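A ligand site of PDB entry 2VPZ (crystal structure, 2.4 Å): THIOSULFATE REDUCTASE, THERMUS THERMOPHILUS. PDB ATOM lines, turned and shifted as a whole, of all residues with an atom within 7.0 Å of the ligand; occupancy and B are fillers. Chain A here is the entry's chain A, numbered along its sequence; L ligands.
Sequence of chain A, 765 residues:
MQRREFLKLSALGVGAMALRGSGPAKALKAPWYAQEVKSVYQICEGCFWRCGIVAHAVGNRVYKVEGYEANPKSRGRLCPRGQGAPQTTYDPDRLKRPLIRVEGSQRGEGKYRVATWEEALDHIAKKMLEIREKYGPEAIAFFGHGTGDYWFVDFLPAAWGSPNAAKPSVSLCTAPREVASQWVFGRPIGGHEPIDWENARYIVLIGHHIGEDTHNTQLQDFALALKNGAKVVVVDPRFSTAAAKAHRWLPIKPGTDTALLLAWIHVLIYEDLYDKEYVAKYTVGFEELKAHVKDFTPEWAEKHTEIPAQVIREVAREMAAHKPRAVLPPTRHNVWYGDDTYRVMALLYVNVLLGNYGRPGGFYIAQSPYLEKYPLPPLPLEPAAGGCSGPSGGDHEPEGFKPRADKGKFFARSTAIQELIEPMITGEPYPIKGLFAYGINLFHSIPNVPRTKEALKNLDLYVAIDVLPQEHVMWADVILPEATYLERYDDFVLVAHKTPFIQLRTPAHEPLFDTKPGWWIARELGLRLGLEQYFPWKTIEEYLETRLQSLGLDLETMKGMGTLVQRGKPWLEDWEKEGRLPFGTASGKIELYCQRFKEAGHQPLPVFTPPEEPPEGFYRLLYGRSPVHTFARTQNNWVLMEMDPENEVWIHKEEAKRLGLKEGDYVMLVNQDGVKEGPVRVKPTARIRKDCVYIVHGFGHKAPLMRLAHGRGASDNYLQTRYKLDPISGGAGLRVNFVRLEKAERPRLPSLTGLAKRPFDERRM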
ATOM      1  N   ILE A  43      17.511  26.796  10.487  1.00  0.00           N
ATOM      2  CA  ILE A  43      18.328  26.109  11.493  1.00  0.00           C
ATOM      3  C   ILE A  43      18.508  24.616  11.146  1.00  0.00           C
ATOM      4  O   ILE A  43      17.607  24.008  10.591  1.00  0.00           O
ATOM      5  CB  ILE A  43      17.626  26.174  12.908  1.00  0.00           C
ATOM      6  CG1 ILE A  43      16.942  27.523  13.084  1.00  0.00           C
ATOM      7  CG2 ILE A  43      18.635  25.913  14.024  1.00  0.00           C
ATOM      8  CD1 ILE A  43      16.939  28.075  14.530  1.00  0.00           C
ATOM      9  N   CYS A  44      19.658  24.023  11.452  1.00  0.00           N
ATOM     10  CA  CYS A  44      19.874  22.581  11.197  1.00  0.00           C
ATOM     11  C   CYS A  44      19.353  21.775  12.423  1.00  0.00           C
ATOM     12  O   CYS A  44      19.677  22.122  13.558  1.00  0.00           O
ATOM     13  CB  CYS A  44      21.379  22.264  10.957  1.00  0.00           C
ATOM     14  SG  CYS A  44      21.848  20.492  11.011  1.00  0.00           S
ATOM     15  N   GLU A  45      18.514  20.755  12.222  1.00  0.00           N
ATOM     16  CA  GLU A  45      18.049  19.904  13.336  1.00  0.00           C
ATOM     17  C   GLU A  45      18.907  18.579  13.322  1.00  0.00           C
ATOM     18  O   GLU A  45      18.591  17.607  13.998  1.00  0.00           O
ATOM     19  CB  GLU A  45      16.511  19.620  13.303  1.00  0.00           C
ATOM     20  CG  GLU A  45      15.852  19.168  14.672  1.00  0.00           C
ATOM     21  CD  GLU A  45      16.019  20.166  15.849  1.00  0.00           C
ATOM     22  OE1 GLU A  45      16.028  21.390  15.602  1.00  0.00           O
ATOM     23  OE2 GLU A  45      16.132  19.709  17.031  1.00  0.00           O
ATOM     24  N   GLY A  46      19.997  18.599  12.540  1.00  0.00           N
ATOM     25  CA  GLY A  46      20.952  17.508  12.453  1.00  0.00           C
ATOM     26  C   GLY A  46      21.418  17.001  13.830  1.00  0.00           C
ATOM     27  O   GLY A  46      21.600  15.778  14.030  1.00  0.00           O
ATOM     28  N   CYS A  47      21.622  17.906  14.778  1.00  0.00           N
ATOM     29  CA  CYS A  47      21.977  17.612  16.168  1.00  0.00           C
ATOM     30  C   CYS A  47      21.643  18.863  17.022  1.00  0.00           C
ATOM     31  O   CYS A  47      21.048  19.814  16.508  1.00  0.00           O
ATOM     32  CB  CYS A  47      23.451  17.208  16.332  1.00  0.00           C
ATOM     33  SG  CYS A  47      24.723  18.570  16.283  1.00  0.00           S
ATOM     34  N   PHE A  48      22.035  18.904  18.282  1.00  0.00           N
ATOM     35  CA  PHE A  48      21.658  20.029  19.095  1.00  0.00           C
ATOM     36  C   PHE A  48      22.533  21.283  19.016  1.00  0.00           C
ATOM     37  O   PHE A  48      22.254  22.279  19.669  1.00  0.00           O
ATOM     38  CB  PHE A  48      21.464  19.517  20.561  1.00  0.00           C
ATOM     39  CG  PHE A  48      20.658  18.192  20.653  1.00  0.00           C
ATOM     40  CD1 PHE A  48      21.071  17.142  21.485  1.00  0.00           C
ATOM     41  CD2 PHE A  48      19.524  18.015  19.848  1.00  0.00           C
ATOM     42  CE1 PHE A  48      20.344  15.910  21.491  1.00  0.00           C
ATOM     43  CE2 PHE A  48      18.786  16.779  19.863  1.00  0.00           C
ATOM     44  CZ  PHE A  48      19.197  15.738  20.675  1.00  0.00           C
ATOM     45  N   TRP A  49      23.560  21.280  18.172  1.00  0.00           N
ATOM     46  CA  TRP A  49      24.435  22.462  18.041  1.00  0.00           C
ATOM     47  C   TRP A  49      23.626  23.646  17.447  1.00  0.00           C
ATOM     48  O   TRP A  49      23.950  24.822  17.673  1.00  0.00           O
ATOM     49  CB  TRP A  49      25.669  22.144  17.212  1.00  0.00           C
ATOM     50  CG  TRP A  49      26.859  23.096  17.403  1.00  0.00           C
ATOM     51  CD1 TRP A  49      27.367  23.976  16.479  1.00  0.00           C
ATOM     52  CD2 TRP A  49      27.729  23.194  18.560  1.00  0.00           C
ATOM     53  NE1 TRP A  49      28.481  24.594  16.982  1.00  0.00           N
ATOM     54  CE2 TRP A  49      28.733  24.146  18.245  1.00  0.00           C
ATOM     55  CE3 TRP A  49      27.770  22.562  19.810  1.00  0.00           C
ATOM     56  CZ2 TRP A  49      29.751  24.503  19.161  1.00  0.00           C
ATOM     57  CZ3 TRP A  49      28.791  22.925  20.733  1.00  0.00           C
ATOM     58  CH2 TRP A  49      29.767  23.879  20.388  1.00  0.00           C
ATOM     59  N   ARG A  50      22.600  23.283  16.678  1.00  0.00           N
ATOM     60  CA  ARG A  50      21.646  24.167  15.985  1.00  0.00           C
ATOM     61  C   ARG A  50      22.296  25.257  15.070  1.00  0.00           C
ATOM     62  O   ARG A  50      22.029  26.448  15.212  1.00  0.00           O
ATOM     63  CB  ARG A  50      20.650  24.753  17.020  1.00  0.00           C
ATOM     64  CG  ARG A  50      19.743  23.685  17.774  1.00  0.00           C
ATOM     65  CD  ARG A  50      18.891  24.222  18.977  1.00  0.00           C
ATOM     66  NE  ARG A  50      19.323  23.727  20.290  1.00  0.00           N
ATOM     67  CZ  ARG A  50      18.754  22.765  21.007  1.00  0.00           C
ATOM     68  NH1 ARG A  50      17.658  22.138  20.586  1.00  0.00           N
ATOM     69  NH2 ARG A  50      19.289  22.382  22.181  1.00  0.00           N
ATOM     70  N   CYS A  51      23.159  24.842  14.133  1.00  0.00           N
ATOM     71  CA  CYS A  51      23.834  25.765  13.194  1.00  0.00           C
ATOM     72  C   CYS A  51      22.796  26.485  12.289  1.00  0.00           C
ATOM     73  O   CYS A  51      21.767  25.902  11.925  1.00  0.00           O
ATOM     74  CB  CYS A  51      24.879  25.040  12.292  1.00  0.00           C
ATOM     75  SG  CYS A  51      26.105  23.969  13.124  1.00  0.00           S
ATOM     76  N   GLY A  52      23.079  27.754  11.989  1.00  0.00           N
ATOM     77  CA  GLY A  52      22.256  28.553  11.099  1.00  0.00           C
ATOM     78  C   GLY A  52      22.633  28.153   9.671  1.00  0.00           C
ATOM     79  O   GLY A  52      23.825  28.098   9.346  1.00  0.00           O
ATOM     80  N   ILE A  53      21.642  27.865   8.837  1.00  0.00           N
ATOM     81  CA  ILE A  53      21.817  27.423   7.455  1.00  0.00           C
ATOM     82  C   ILE A  53      20.859  28.061   6.444  1.00  0.00           C
ATOM     83  O   ILE A  53      19.823  28.630   6.809  1.00  0.00           O
ATOM     84  CB  ILE A  53      21.607  25.849   7.341  1.00  0.00           C
ATOM     85  CG1 ILE A  53      20.233  25.444   7.855  1.00  0.00           C
ATOM     86  CG2 ILE A  53      22.725  25.085   8.092  1.00  0.00           C
ATOM     87  CD1 ILE A  53      19.608  24.197   7.249  1.00  0.00           C
ATOM     88  N   LYS A  73      27.798  30.371  14.312  1.00  0.00           N
ATOM     89  CA  LYS A  73      27.958  28.917  14.410  1.00  0.00           C
ATOM     90  C   LYS A  73      28.509  28.277  13.129  1.00  0.00           C
ATOM     91  O   LYS A  73      29.569  27.659  13.138  1.00  0.00           O
ATOM     92  CB  LYS A  73      26.640  28.238  14.838  1.00  0.00           C
ATOM     93  CG  LYS A  73      26.236  28.475  16.289  1.00  0.00           C
ATOM     94  CD  LYS A  73      25.191  27.484  16.739  1.00  0.00           C
ATOM     95  CE  LYS A  73      24.982  27.473  18.252  1.00  0.00           C
ATOM     96  NZ  LYS A  73      25.894  26.504  18.951  1.00  0.00           N
ATOM     97  N   SER A  74      27.821  28.443  11.999  1.00  0.00           N
ATOM     98  CA  SER A  74      28.333  27.870  10.748  1.00  0.00           C
ATOM     99  C   SER A  74      29.453  28.686  10.051  1.00  0.00           C
ATOM    100  O   SER A  74      30.439  28.107   9.579  1.00  0.00           O
ATOM    101  CB  SER A  74      27.190  27.596   9.752  1.00  0.00           C
ATOM    102  OG  SER A  74      26.267  28.643   9.668  1.00  0.00           O
ATOM    103  N   ARG A  77      30.550  27.292   6.632  1.00  0.00           N
ATOM    104  CA  ARG A  77      30.800  25.842   6.617  1.00  0.00           C
ATOM    105  C   ARG A  77      29.652  24.995   7.229  1.00  0.00           C
ATOM    106  O   ARG A  77      28.693  25.522   7.828  1.00  0.00           O
ATOM    107  CB  ARG A  77      32.104  25.476   7.352  1.00  0.00           C
ATOM    108  CG  ARG A  77      33.145  26.558   7.532  1.00  0.00           C
ATOM    109  CD  ARG A  77      34.022  26.699   6.307  1.00  0.00           C
ATOM    110  NE  ARG A  77      33.532  27.710   5.377  1.00  0.00           N
ATOM    111  CZ  ARG A  77      34.117  28.875   5.161  1.00  0.00           C
ATOM    112  NH1 ARG A  77      35.223  29.163   5.817  1.00  0.00           N
ATOM    113  NH2 ARG A  77      33.610  29.754   4.307  1.00  0.00           N
ATOM    114  N   LEU A  78      29.764  23.672   7.075  1.00  0.00           N
ATOM    115  CA  LEU A  78      28.807  22.669   7.549  1.00  0.00           C
ATOM    116  C   LEU A  78      29.499  21.288   7.659  1.00  0.00           C
ATOM    117  O   LEU A  78      30.351  20.936   6.826  1.00  0.00           O
ATOM    118  CB  LEU A  78      27.600  22.581   6.566  1.00  0.00           C
ATOM    119  CG  LEU A  78      26.137  22.643   7.081  1.00  0.00           C
ATOM    120  CD1 LEU A  78      25.970  23.840   8.068  1.00  0.00           C
ATOM    121  CD2 LEU A  78      25.132  22.774   5.905  1.00  0.00           C
ATOM    122  N   CYS A  79      29.153  20.510   8.698  1.00  0.00           N
ATOM    123  CA  CYS A  79      29.707  19.177   8.886  1.00  0.00           C
ATOM    124  C   CYS A  79      28.895  18.203   8.001  1.00  0.00           C
ATOM    125  O   CYS A  79      27.852  18.574   7.458  1.00  0.00           O
ATOM    126  CB  CYS A  79      29.601  18.734  10.378  1.00  0.00           C
ATOM    127  SG  CYS A  79      27.941  18.019  10.925  1.00  0.00           S
ATOM    128  N   PRO A  80      29.361  16.936   7.844  1.00  0.00           N
ATOM    129  CA  PRO A  80      28.663  15.917   7.039  1.00  0.00           C
ATOM    130  C   PRO A  80      27.169  15.680   7.402  1.00  0.00           C
ATOM    131  O   PRO A  80      26.292  15.568   6.535  1.00  0.00           O
ATOM    132  CB  PRO A  80      29.534  14.661   7.183  1.00  0.00           C
ATOM    133  CG  PRO A  80      30.278  14.887   8.513  1.00  0.00           C
ATOM    134  CD  PRO A  80      30.513  16.370   8.567  1.00  0.00           C
ATOM    135  N   ARG A  81      26.880  15.607   8.699  1.00  0.00           N
ATOM    136  CA  ARG A  81      25.516  15.399   9.212  1.00  0.00           C
ATOM    137  C   ARG A  81      24.572  16.536   8.815  1.00  0.00           C
ATOM    138  O   ARG A  81      23.384  16.300   8.553  1.00  0.00           O
ATOM    139  CB  ARG A  81      25.547  15.203  10.740  1.00  0.00           C
ATOM    140  CG  ARG A  81      26.239  13.887  11.126  1.00  0.00           C
ATOM    141  CD  ARG A  81      26.663  13.812  12.605  1.00  0.00           C
ATOM    142  NE  ARG A  81      27.431  14.953  13.082  1.00  0.00           N
ATOM    143  CZ  ARG A  81      27.039  15.834  14.009  1.00  0.00           C
ATOM    144  NH1 ARG A  81      25.852  15.720  14.582  1.00  0.00           N
ATOM    145  NH2 ARG A  81      27.832  16.860  14.321  1.00  0.00           N
ATOM    146  N   GLY A  82      25.088  17.769   8.767  1.00  0.00           N
ATOM    147  CA  GLY A  82      24.294  18.909   8.368  1.00  0.00           C
ATOM    148  C   GLY A  82      23.945  18.823   6.890  1.00  0.00           C
ATOM    149  O   GLY A  82      22.804  19.112   6.475  1.00  0.00           O
ATOM    150  N   GLN A  83      24.923  18.405   6.082  1.00  0.00           N
ATOM    151  CA  GLN A  83      24.742  18.250   4.626  1.00  0.00           C
ATOM    152  C   GLN A  83      23.746  17.145   4.223  1.00  0.00           C
ATOM    153  O   GLN A  83      22.962  17.327   3.291  1.00  0.00           O
ATOM    154  CB  GLN A  83      26.085  18.005   3.905  1.00  0.00           C
ATOM    155  CG  GLN A  83      27.131  19.153   3.945  1.00  0.00           C
ATOM    156  CD  GLN A  83      26.851  20.314   2.974  1.00  0.00           C
ATOM    157  OE1 GLN A  83      27.565  21.315   2.944  1.00  0.00           O
ATOM    158  NE2 GLN A  83      25.788  20.169   2.165  1.00  0.00           N
ATOM    159  N   ALA A  85      21.416  15.731   6.404  1.00  0.00           N
ATOM    160  CA  ALA A  85      20.176  15.847   7.212  1.00  0.00           C
ATOM    161  C   ALA A  85      18.832  15.953   6.462  1.00  0.00           C
ATOM    162  O   ALA A  85      17.822  15.451   6.917  1.00  0.00           O
ATOM    163  CB  ALA A  85      20.305  17.009   8.270  1.00  0.00           C
ATOM    164  N   THR A 214      31.753  15.790  15.839  1.00  0.00           N
ATOM    165  CA  THR A 214      31.875  16.699  14.739  1.00  0.00           C
ATOM    166  C   THR A 214      31.074  18.017  14.733  1.00  0.00           C
ATOM    167  O   THR A 214      30.730  18.576  13.670  1.00  0.00           O
ATOM    168  CB  THR A 214      31.704  15.782  13.455  1.00  0.00           C
ATOM    169  OG1 THR A 214      32.731  16.035  12.510  1.00  0.00           O
ATOM    170  CG2 THR A 214      30.329  15.881  12.850  1.00  0.00           C
ATOM    171  N   HIS A 215      30.790  18.506  15.962  1.00  0.00           N
ATOM    172  CA  HIS A 215      30.092  19.794  16.236  1.00  0.00           C
ATOM    173  C   HIS A 215      30.871  20.822  15.395  1.00  0.00           C
ATOM    174  O   HIS A 215      32.072  21.030  15.564  1.00  0.00           O
ATOM    175  CB  HIS A 215      30.111  20.152  17.764  1.00  0.00           C
ATOM    176  CG  HIS A 215      28.980  19.606  18.560  1.00  0.00           C
ATOM    177  ND1 HIS A 215      28.998  19.466  19.922  1.00  0.00           N
ATOM    178  CD2 HIS A 215      27.787  19.158  18.158  1.00  0.00           C
ATOM    179  CE1 HIS A 215      27.860  18.929  20.328  1.00  0.00           C
ATOM    180  NE2 HIS A 215      27.114  18.733  19.264  1.00  0.00           N
ATOM    181  N   ASN A 216      30.106  21.436  14.508  1.00  0.00           N
ATOM    182  CA  ASN A 216      30.653  22.403  13.564  1.00  0.00           C
ATOM    183  C   ASN A 216      31.731  23.387  14.001  1.00  0.00           C
ATOM    184  O   ASN A 216      32.929  23.195  13.717  1.00  0.00           O
ATOM    185  CB  ASN A 216      29.536  23.185  12.880  1.00  0.00           C
ATOM    186  CG  ASN A 216      29.968  23.842  11.583  1.00  0.00           C
ATOM    187  OD1 ASN A 216      31.163  23.850  11.287  1.00  0.00           O
ATOM    188  ND2 ASN A 216      29.018  24.369  10.813  1.00  0.00           N
ATOM    189  N   THR A 217      31.317  24.426  14.710  1.00  0.00           N
ATOM    190  CA  THR A 217      32.197  25.510  15.142  1.00  0.00           C
ATOM    191  C   THR A 217      33.434  25.093  15.922  1.00  0.00           C
ATOM    192  O   THR A 217      34.527  25.681  15.757  1.00  0.00           O
ATOM    193  CB  THR A 217      31.451  26.610  15.993  1.00  0.00           C
ATOM    194  OG1 THR A 217      30.092  26.686  15.607  1.00  0.00           O
ATOM    195  CG2 THR A 217      32.130  27.982  15.810  1.00  0.00           C
ATOM    196  N   THR A 630      24.500  10.791  13.504  1.00  0.00           N
ATOM    197  CA  THR A 630      24.102  11.434  14.754  1.00  0.00           C
ATOM    198  C   THR A 630      23.501  10.307  15.691  1.00  0.00           C
ATOM    199  O   THR A 630      22.747   9.471  15.202  1.00  0.00           O
ATOM    200  CB  THR A 630      23.043  12.566  14.497  1.00  0.00           C
ATOM    201  OG1 THR A 630      23.640  13.633  13.736  1.00  0.00           O
ATOM    202  CG2 THR A 630      22.517  13.123  15.837  1.00  0.00           C
HETATM  203 FE1  LIG L   1      25.465  21.833  12.986  1.00  0.00          FE
HETATM  204 FE2  LIG L   1      26.528  19.480  12.047  1.00  0.00          FE
HETATM  205 FE3  LIG L   1      24.811  19.500  14.189  1.00  0.00          FE
HETATM  206 FE4  LIG L   1      23.840  20.019  11.683  1.00  0.00          FE
HETATM  207  S1  LIG L   1      24.773  18.038  12.385  1.00  0.00           S
HETATM  208  S2  LIG L   1      23.347  21.187  13.631  1.00  0.00           S
HETATM  209  S3  LIG L   1      25.607  21.152  10.768  1.00  0.00           S
HETATM  210  S4  LIG L   1      26.931  20.437  14.115  1.00  0.00           S
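SG of Cys 44 binds FE4 of the ligand (2.2 Å).
The backbone NH (N) of Cys 51 lies close to a sulfur (S2) of the ligand (3.7 Å).
An iron atom (FE1) of the ligand is bound by the side-chain sulfur of Cys 51 (2.2 Å).
An iron atom (FE3) of the ligand is bound by the side-chain sulfur (SG) of Cys 47 (2.3 Å).
An iron atom (FE2) of the ligand is bound by the side-chain sulfur (SG) of Cys 79, 2.3 Å away.
A sulfur (S4) of the ligand sits close to the backbone NH of Asn 216 (3.4 Å).
The guanidinium group (NH1) of Arg 81 lies close to a sulfur (S1) of the ligand.
S1 of the ligand lies close to N of Gly 82 (3.6 Å).
A sulfur (S2) of the ligand sits close to the backbone NH (N) of Arg 50 (3.8 Å).
Gly 46 touches the ligand (C to S1, 3.8 Å).
Trp 49 touches the ligand (CB to S4, 3.8 Å).
Leu 78 touches the ligand (CD1 to S3, 3.8 Å).
CA of His 215 touches S4 of the ligand (3.9 Å).
Hydrophobic or aromatic side chains within 4 Å of the ligand: Trp 49 and Leu 78.
Within 4 Å of the ligand: Cys 44, Gly 46, Cys 47, Trp 49, Arg 50, Cys 51, Leu 78, Cys 79, Arg 81, Gly 82, His 215 and Asn 216.
The nearest printed residue that does not touch the ligand is Thr 214 (4.3 Å).
The side-chain sulfur (SG) of Cys 47 lies close to the guanidinium group (NH1) of Arg 81, 3.5 Å away.
SG of Cys 47 sits close to N of Trp 49, at 3.5 Å.
The side-chain sulfur (SG) of Cys 79 sits close to the backbone NH (N) of Gly 82 (3.6 Å).
The side-chain amide nitrogen (ND2) of Asn 216 sits at hydrogen-bond distance from the backbone carbonyl oxygen (O) of Arg 77 (3.2 Å).
O of Thr 214 sits close to NH2 of Arg 81.
The guanidinium group of Arg 81 lies within hydrogen-bond range of the side-chain hydroxyl of Thr 630, 3.2 Å away.
OG1 of Thr 217 sits at hydrogen-bond distance from NE1 of Trp 49, 3.0 Å away.
The backbone carbonyl oxygen (O) of Trp 49 sits at hydrogen-bond distance from the side-chain amino group (NZ) of Lys 73, 2.9 Å away.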
